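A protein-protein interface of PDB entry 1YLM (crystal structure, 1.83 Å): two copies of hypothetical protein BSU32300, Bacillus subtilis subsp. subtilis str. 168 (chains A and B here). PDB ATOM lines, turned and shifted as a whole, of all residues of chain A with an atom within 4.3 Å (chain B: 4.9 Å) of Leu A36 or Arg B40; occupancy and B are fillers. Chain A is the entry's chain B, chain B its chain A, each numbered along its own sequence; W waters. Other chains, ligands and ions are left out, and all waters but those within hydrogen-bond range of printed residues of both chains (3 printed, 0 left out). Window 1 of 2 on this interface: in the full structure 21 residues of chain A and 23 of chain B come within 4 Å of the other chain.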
ATOM      1  N   GLU A  32      17.957  -8.427 -10.219  1.00  0.00           N
ATOM      2  CA  GLU A  32      19.202  -7.860  -9.669  1.00  0.00           C
ATOM      3  C   GLU A  32      19.949  -7.000 -10.700  1.00  0.00           C
ATOM      4  O   GLU A  32      20.383  -5.884 -10.394  1.00  0.00           O
ATOM      5  CB  GLU A  32      20.098  -8.965  -9.113  1.00  0.00           C
ATOM      6  CG  GLU A  32      19.493  -9.679  -7.902  1.00  0.00           C
ATOM      7  CD  GLU A  32      20.073  -9.237  -6.572  1.00  0.00           C
ATOM      8  OE1 GLU A  32      20.658  -8.123  -6.474  1.00  0.00           O
ATOM      9  OE2 GLU A  32      19.941 -10.026  -5.608  1.00  0.00           O
ATOM     10  N   ILE A  33      20.053  -7.505 -11.924  1.00  0.00           N
ATOM     11  CA  ILE A  33      20.656  -6.747 -13.032  1.00  0.00           C
ATOM     12  C   ILE A  33      19.767  -5.568 -13.441  1.00  0.00           C
ATOM     13  O   ILE A  33      20.258  -4.463 -13.650  1.00  0.00           O
ATOM     14  CB  ILE A  33      20.995  -7.679 -14.221  1.00  0.00           C
ATOM     15  CG1 ILE A  33      21.999  -8.758 -13.765  1.00  0.00           C
ATOM     16  CG2 ILE A  33      21.460  -6.900 -15.472  1.00  0.00           C
ATOM     17  CD1 ILE A  33      23.331  -8.230 -13.158  1.00  0.00           C
ATOM     18  N   GLY A  34      18.453  -5.790 -13.516  1.00  0.00           N
ATOM     19  CA  GLY A  34      17.528  -4.730 -13.922  1.00  0.00           C
ATOM     20  C   GLY A  34      17.590  -3.540 -12.973  1.00  0.00           C
ATOM     21  O   GLY A  34      17.607  -2.394 -13.416  1.00  0.00           O
ATOM     22  N   GLU A  35      17.647  -3.827 -11.675  1.00  0.00           N
ATOM     23  CA  GLU A  35      17.708  -2.796 -10.629  1.00  0.00           C
ATOM     24  C   GLU A  35      18.921  -1.905 -10.846  1.00  0.00           C
ATOM     25  O   GLU A  35      18.823  -0.691 -10.753  1.00  0.00           O
ATOM     26  CB  GLU A  35      17.844  -3.449  -9.252  1.00  0.00           C
ATOM     27  CG  GLU A  35      16.539  -3.906  -8.646  1.00  0.00           C
ATOM     28  CD  GLU A  35      16.753  -4.535  -7.280  1.00  0.00           C
ATOM     29  OE1 GLU A  35      17.922  -4.827  -6.933  1.00  0.00           O
ATOM     30  OE2 GLU A  35      15.752  -4.737  -6.556  1.00  0.00           O
ATOM     31  N   LEU A  36      20.047  -2.530 -11.178  1.00  0.00           N
ATOM     32  CA  LEU A  36      21.296  -1.790 -11.376  1.00  0.00           C
ATOM     33  C   LEU A  36      21.215  -0.925 -12.629  1.00  0.00           C
ATOM     34  O   LEU A  36      21.670   0.209 -12.625  1.00  0.00           O
ATOM     35  CB  LEU A  36      22.471  -2.747 -11.491  1.00  0.00           C
ATOM     36  CG  LEU A  36      22.918  -3.411 -10.188  1.00  0.00           C
ATOM     37  CD1 LEU A  36      23.669  -4.676 -10.555  1.00  0.00           C
ATOM     38  CD2 LEU A  36      23.774  -2.464  -9.343  1.00  0.00           C
ATOM     39  N   ALA A  37      20.639  -1.490 -13.688  1.00  0.00           N
ATOM     40  CA  ALA A  37      20.493  -0.788 -14.960  1.00  0.00           C
ATOM     41  C   ALA A  37      19.630   0.454 -14.753  1.00  0.00           C
ATOM     42  O   ALA A  37      19.974   1.532 -15.235  1.00  0.00           O
ATOM     43  CB  ALA A  37      19.873  -1.722 -16.012  1.00  0.00           C
ATOM     44  N   LEU A  38      18.511   0.311 -14.035  1.00  0.00           N
ATOM     45  CA  LEU A  38      17.608   1.450 -13.826  1.00  0.00           C
ATOM     46  C   LEU A  38      18.296   2.556 -13.021  1.00  0.00           C
ATOM     47  O   LEU A  38      18.135   3.754 -13.326  1.00  0.00           O
ATOM     48  CB  LEU A  38      16.323   1.012 -13.132  1.00  0.00           C
ATOM     49  CG  LEU A  38      15.291   2.133 -12.987  1.00  0.00           C
ATOM     50  CD1 LEU A  38      14.920   2.724 -14.355  1.00  0.00           C
ATOM     51  CD2 LEU A  38      14.083   1.549 -12.290  1.00  0.00           C
ATOM     52  N   GLN A  39      19.061   2.161 -11.993  1.00  0.00           N
ATOM     53  CA  GLN A  39      19.867   3.148 -11.229  1.00  0.00           C
ATOM     54  C   GLN A  39      20.800   3.940 -12.141  1.00  0.00           C
ATOM     55  O   GLN A  39      20.903   5.158 -12.013  1.00  0.00           O
ATOM     56  CB  GLN A  39      20.664   2.484 -10.114  1.00  0.00           C
ATOM     57  CG  GLN A  39      19.757   1.947  -8.988  1.00  0.00           C
ATOM     58  CD  GLN A  39      20.492   1.120  -7.950  1.00  0.00           C
ATOM     59  OE1 GLN A  39      21.726   1.100  -7.894  1.00  0.00           O
ATOM     60  NE2 GLN A  39      19.728   0.432  -7.116  1.00  0.00           N
ATOM     61  N   ARG A  40      21.465   3.254 -13.062  1.00  0.00           N
ATOM     62  CA  ARG A  40      22.370   3.924 -14.008  1.00  0.00           C
ATOM     63  C   ARG A  40      21.570   4.887 -14.885  1.00  0.00           C
ATOM     64  O   ARG A  40      21.960   6.051 -15.082  1.00  0.00           O
ATOM     65  CB  ARG A  40      23.138   2.910 -14.871  1.00  0.00           C
ATOM     66  CG  ARG A  40      24.207   3.577 -15.796  1.00  0.00           C
ATOM     67  CD  ARG A  40      25.311   4.240 -14.992  1.00  0.00           C
ATOM     68  NE  ARG A  40      26.313   4.867 -15.865  1.00  0.00           N
ATOM     69  CZ  ARG A  40      27.230   5.741 -15.451  1.00  0.00           C
ATOM     70  NH1 ARG A  40      27.300   6.094 -14.164  1.00  0.00           N
ATOM     71  NH2 ARG A  40      28.083   6.271 -16.336  1.00  0.00           N
ATOM     72  N   LEU A  99      21.351   8.387  -5.309  1.00  0.00           N
ATOM     73  CA  LEU A  99      22.055   7.628  -6.334  1.00  0.00           C
ATOM     74  C   LEU A  99      23.575   7.755  -6.292  1.00  0.00           C
ATOM     75  O   LEU A  99      24.291   6.778  -6.551  1.00  0.00           O
ATOM     76  CB  LEU A  99      21.532   7.989  -7.725  1.00  0.00           C
ATOM     77  CG  LEU A  99      20.118   7.500  -8.044  1.00  0.00           C
ATOM     78  CD1 LEU A  99      19.572   8.273  -9.266  1.00  0.00           C
ATOM     79  CD2 LEU A  99      20.103   5.984  -8.289  1.00  0.00           C
ATOM     80  N   TYR A 103      24.174   5.655  -1.639  1.00  0.00           N
ATOM     81  CA  TYR A 103      23.807   4.568  -2.552  1.00  0.00           C
ATOM     82  C   TYR A 103      23.394   3.279  -1.846  1.00  0.00           C
ATOM     83  O   TYR A 103      22.751   2.415  -2.464  1.00  0.00           O
ATOM     84  CB  TYR A 103      24.930   4.336  -3.582  1.00  0.00           C
ATOM     85  CG  TYR A 103      26.293   4.188  -2.929  1.00  0.00           C
ATOM     86  CD1 TYR A 103      26.697   2.962  -2.389  1.00  0.00           C
ATOM     87  CD2 TYR A 103      27.167   5.270  -2.841  1.00  0.00           C
ATOM     88  CE1 TYR A 103      27.937   2.820  -1.769  1.00  0.00           C
ATOM     89  CE2 TYR A 103      28.415   5.145  -2.239  1.00  0.00           C
ATOM     90  CZ  TYR A 103      28.790   3.916  -1.709  1.00  0.00           C
ATOM     91  OH  TYR A 103      30.012   3.784  -1.116  1.00  0.00           O
ATOM     92  N   GLN B  19      27.616  -6.576  -4.873  1.00  0.00           N
ATOM     93  CA  GLN B  19      27.801  -6.087  -6.253  1.00  0.00           C
ATOM     94  C   GLN B  19      28.880  -6.910  -6.978  1.00  0.00           C
ATOM     95  O   GLN B  19      28.735  -7.225  -8.178  1.00  0.00           O
ATOM     96  CB  GLN B  19      28.160  -4.601  -6.313  1.00  0.00           C
ATOM     97  CG  GLN B  19      27.307  -3.590  -5.482  1.00  0.00           C
ATOM     98  CD  GLN B  19      25.820  -3.923  -5.383  1.00  0.00           C
ATOM     99  OE1 GLN B  19      25.280  -4.061  -4.284  1.00  0.00           O
ATOM    100  NE2 GLN B  19      25.163  -4.040  -6.505  1.00  0.00           N
ATOM    101  N   LEU B  22      27.424 -10.111  -8.089  1.00  0.00           N
ATOM    102  CA  LEU B  22      26.593  -9.885  -9.267  1.00  0.00           C
ATOM    103  C   LEU B  22      27.471  -9.779 -10.504  1.00  0.00           C
ATOM    104  O   LEU B  22      27.128 -10.328 -11.559  1.00  0.00           O
ATOM    105  CB  LEU B  22      25.723  -8.636  -9.088  1.00  0.00           C
ATOM    106  CG  LEU B  22      24.597  -8.766  -8.059  1.00  0.00           C
ATOM    107  CD1 LEU B  22      23.818  -7.465  -7.914  1.00  0.00           C
ATOM    108  CD2 LEU B  22      23.648  -9.922  -8.428  1.00  0.00           C
ATOM    109  N   LEU B  36      24.476  -0.996 -19.033  1.00  0.00           N
ATOM    110  CA  LEU B  36      24.060  -0.038 -18.029  1.00  0.00           C
ATOM    111  C   LEU B  36      24.280  -0.610 -16.637  1.00  0.00           C
ATOM    112  O   LEU B  36      24.793   0.091 -15.768  1.00  0.00           O
ATOM    113  CB  LEU B  36      22.592   0.309 -18.225  1.00  0.00           C
ATOM    114  CG  LEU B  36      22.280   1.263 -19.379  1.00  0.00           C
ATOM    115  CD1 LEU B  36      20.768   1.186 -19.609  1.00  0.00           C
ATOM    116  CD2 LEU B  36      22.721   2.684 -19.041  1.00  0.00           C
ATOM    117  N   ALA B  37      23.906  -1.880 -16.439  1.00  0.00           N
ATOM    118  CA  ALA B  37      24.106  -2.533 -15.128  1.00  0.00           C
ATOM    119  C   ALA B  37      25.587  -2.586 -14.771  1.00  0.00           C
ATOM    120  O   ALA B  37      25.955  -2.361 -13.616  1.00  0.00           O
ATOM    121  CB  ALA B  37      23.502  -3.938 -15.102  1.00  0.00           C
ATOM    122  N   LEU B  38      26.433  -2.909 -15.748  1.00  0.00           N
ATOM    123  CA  LEU B  38      27.866  -3.010 -15.499  1.00  0.00           C
ATOM    124  C   LEU B  38      28.452  -1.656 -15.133  1.00  0.00           C
ATOM    125  O   LEU B  38      29.291  -1.572 -14.237  1.00  0.00           O
ATOM    126  CB  LEU B  38      28.611  -3.604 -16.697  1.00  0.00           C
ATOM    127  CG  LEU B  38      30.095  -3.895 -16.515  1.00  0.00           C
ATOM    128  CD1 LEU B  38      30.362  -4.847 -15.332  1.00  0.00           C
ATOM    129  CD2 LEU B  38      30.613  -4.473 -17.828  1.00  0.00           C
ATOM    130  N   GLN B  39      27.990  -0.596 -15.781  1.00  0.00           N
ATOM    131  CA  GLN B  39      28.418   0.775 -15.379  1.00  0.00           C
ATOM    132  C   GLN B  39      28.048   1.093 -13.922  1.00  0.00           C
ATOM    133  O   GLN B  39      28.855   1.668 -13.174  1.00  0.00           O
ATOM    134  CB  GLN B  39      27.849   1.844 -16.325  1.00  0.00           C
ATOM    135  CG  GLN B  39      28.461   1.783 -17.745  1.00  0.00           C
ATOM    136  CD  GLN B  39      27.708   2.636 -18.742  1.00  0.00           C
ATOM    137  OE1 GLN B  39      26.914   3.494 -18.366  1.00  0.00           O
ATOM    138  NE2 GLN B  39      27.972   2.418 -20.020  1.00  0.00           N
ATOM    139  N   ARG B  40      26.834   0.715 -13.514  1.00  0.00           N
ATOM    140  CA  ARG B  40      26.429   0.943 -12.128  1.00  0.00           C
ATOM    141  C   ARG B  40      27.300   0.151 -11.155  1.00  0.00           C
ATOM    142  O   ARG B  40      27.747   0.691 -10.146  1.00  0.00           O
ATOM    143  CB  ARG B  40      24.949   0.615 -11.922  1.00  0.00           C
ATOM    144  CG  ARG B  40      24.415   0.937 -10.515  1.00  0.00           C
ATOM    145  CD  ARG B  40      24.462   2.408 -10.220  1.00  0.00           C
ATOM    146  NE  ARG B  40      23.910   2.708  -8.905  1.00  0.00           N
ATOM    147  CZ  ARG B  40      23.978   3.908  -8.331  1.00  0.00           C
ATOM    148  NH1 ARG B  40      24.611   4.907  -8.942  1.00  0.00           N
ATOM    149  NH2 ARG B  40      23.447   4.106  -7.130  1.00  0.00           N
ATOM    150  N   ILE B  41      27.549  -1.119 -11.468  1.00  0.00           N
ATOM    151  CA  ILE B  41      28.429  -1.953 -10.648  1.00  0.00           C
ATOM    152  C   ILE B  41      29.824  -1.315 -10.499  1.00  0.00           C
ATOM    153  O   ILE B  41      30.340  -1.193  -9.369  1.00  0.00           O
ATOM    154  CB  ILE B  41      28.568  -3.394 -11.217  1.00  0.00           C
ATOM    155  CG1 ILE B  41      27.246  -4.167 -11.043  1.00  0.00           C
ATOM    156  CG2 ILE B  41      29.727  -4.120 -10.513  1.00  0.00           C
ATOM    157  CD1 ILE B  41      27.233  -5.496 -11.774  1.00  0.00           C
ATOM    158  N   GLY B  42      30.429  -0.928 -11.622  1.00  0.00           N
ATOM    159  CA  GLY B  42      31.744  -0.251 -11.611  1.00  0.00           C
ATOM    160  C   GLY B  42      31.770   0.964 -10.696  1.00  0.00           C
ATOM    161  O   GLY B  42      32.669   1.102  -9.835  1.00  0.00           O
ATOM    162  N   HIS B  43      30.760   1.819 -10.847  1.00  0.00           N
ATOM    163  CA  HIS B  43      30.597   3.029 -10.035  1.00  0.00           C
ATOM    164  C   HIS B  43      30.503   2.652  -8.555  1.00  0.00           C
ATOM    165  O   HIS B  43      31.257   3.185  -7.720  1.00  0.00           O
ATOM    166  CB  HIS B  43      29.362   3.814 -10.496  1.00  0.00           C
ATOM    167  CG  HIS B  43      29.158   5.113  -9.778  1.00  0.00           C
ATOM    168  ND1 HIS B  43      28.005   5.859  -9.909  1.00  0.00           N
ATOM    169  CD2 HIS B  43      29.965   5.811  -8.940  1.00  0.00           C
ATOM    170  CE1 HIS B  43      28.111   6.960  -9.184  1.00  0.00           C
ATOM    171  NE2 HIS B  43      29.278   6.939  -8.561  1.00  0.00           N
ATOM    172  N   LEU B  44      29.600   1.712  -8.241  1.00  0.00           N
ATOM    173  CA  LEU B  44      29.422   1.268  -6.847  1.00  0.00           C
ATOM    174  C   LEU B  44      30.678   0.660  -6.214  1.00  0.00           C
ATOM    175  O   LEU B  44      30.978   0.960  -5.056  1.00  0.00           O
ATOM    176  CB  LEU B  44      28.218   0.334  -6.711  1.00  0.00           C
ATOM    177  CG  LEU B  44      26.864   0.985  -7.049  1.00  0.00           C
ATOM    178  CD1 LEU B  44      25.750  -0.062  -7.041  1.00  0.00           C
ATOM    179  CD2 LEU B  44      26.535   2.175  -6.122  1.00  0.00           C
HETATM  180  O   HOH W   1      22.840   1.961  -5.263  1.00  0.00           O
HETATM  181  O   HOH W   2      25.894   5.311 -11.685  1.00  0.00           O
HETATM  182  O   HOH W   3      27.469   6.213 -19.195  1.00  0.00           O
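NE of Arg B40 lies within hydrogen-bond range of OE1 of Gln A39, at 2.9 Å.
OE1 of Gln B39 sits at hydrogen-bond distance from NE of Arg A40, at 2.9 Å.
NH2 of Arg B40 lies within hydrogen-bond range of O of Leu A99, 2.9 Å away.
Leu A36 touches six residues of chain B.
Printed residues of chain B within 4 Å of Arg A40: Leu B36 and Gln B39.
Of the printed residues of chain B, Leu A99 touches Arg B40.
Printed residues of chain A within 4 Å of Gln B19: Leu A36 (3.5 Å).
Of the printed residues of chain A, Leu B22 touches Glu A32 (3.5 Å) and Leu A36 (3.8 Å).
Arg B40 touches just these residues of chain A: Leu A36 (3.4 Å), Gln A39 (2.9 Å), Leu A99 (2.9 Å) and Tyr A103 (3.9 Å).
Of the printed residues of chain A, Leu B44 touches Leu A36 (3.9 Å) and Tyr A103 (3.7 Å).
The nearest residue of chain B that does not touch Leu A36 is Leu B36 (4.4 Å).
The nearest printed residue of chain A that does not touch Leu B36 is Ala A37 (4.03 Å).
Of the 11 printed residues of chain B, 8 touch a printed residue of chain A.
Hydrophobic or aromatic side chains of chain B within 4 Å of the printed part of chain A: Leu B22, Leu B36, Ala B37, Ile B41 and Leu B44.
Water W2 lies within hydrogen-bond range of ND1 of His B43, NH1 of Arg A40 and NH1 of Arg B40.
Water W1 lies within hydrogen-bond range of O of Tyr A103, NH2 of Arg B40 and OE1 of Gln A39.
Water W3 lies within hydrogen-bond range of the side-chain amide oxygen of Gln B39 (2.9 Å) and the guanidinium group of Arg A40 (2.9 Å).
Among the printed residues, pairs that only touch across the chains: Leu A36 with Arg B40, Arg A40 with Leu B36, Leu A36 with Gln B19, Glu A32 with Leu B22, Ile A33 with Ala B37, Leu A36 with Ile B41, Tyr A103 with Leu B44, Leu A36 with Leu B22, Tyr A103 with Arg B40, Leu A36 with Leu B44, Ala A37 with Ala B37 and Leu A36 with Ala B37.
Leu A36 touches Ala B37, but with the chains exchanged Ala A37 does not touch Leu B36 (4.03 Å).
Leu A36 touches Arg B40, and with the chains exchanged Arg A40 touches Leu B36.
Ala B37 touches its own counterpart, Ala A37.
Gln A39 touches Arg B40, and with the chains exchanged Arg A40 touches Gln B39.
Positions printed for both chains: 36, 37, 38, 39 and 40.
Of the 15 pairs that touch across the chains among the printed residues, 5 have their exchanged pair printed and touching as well.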
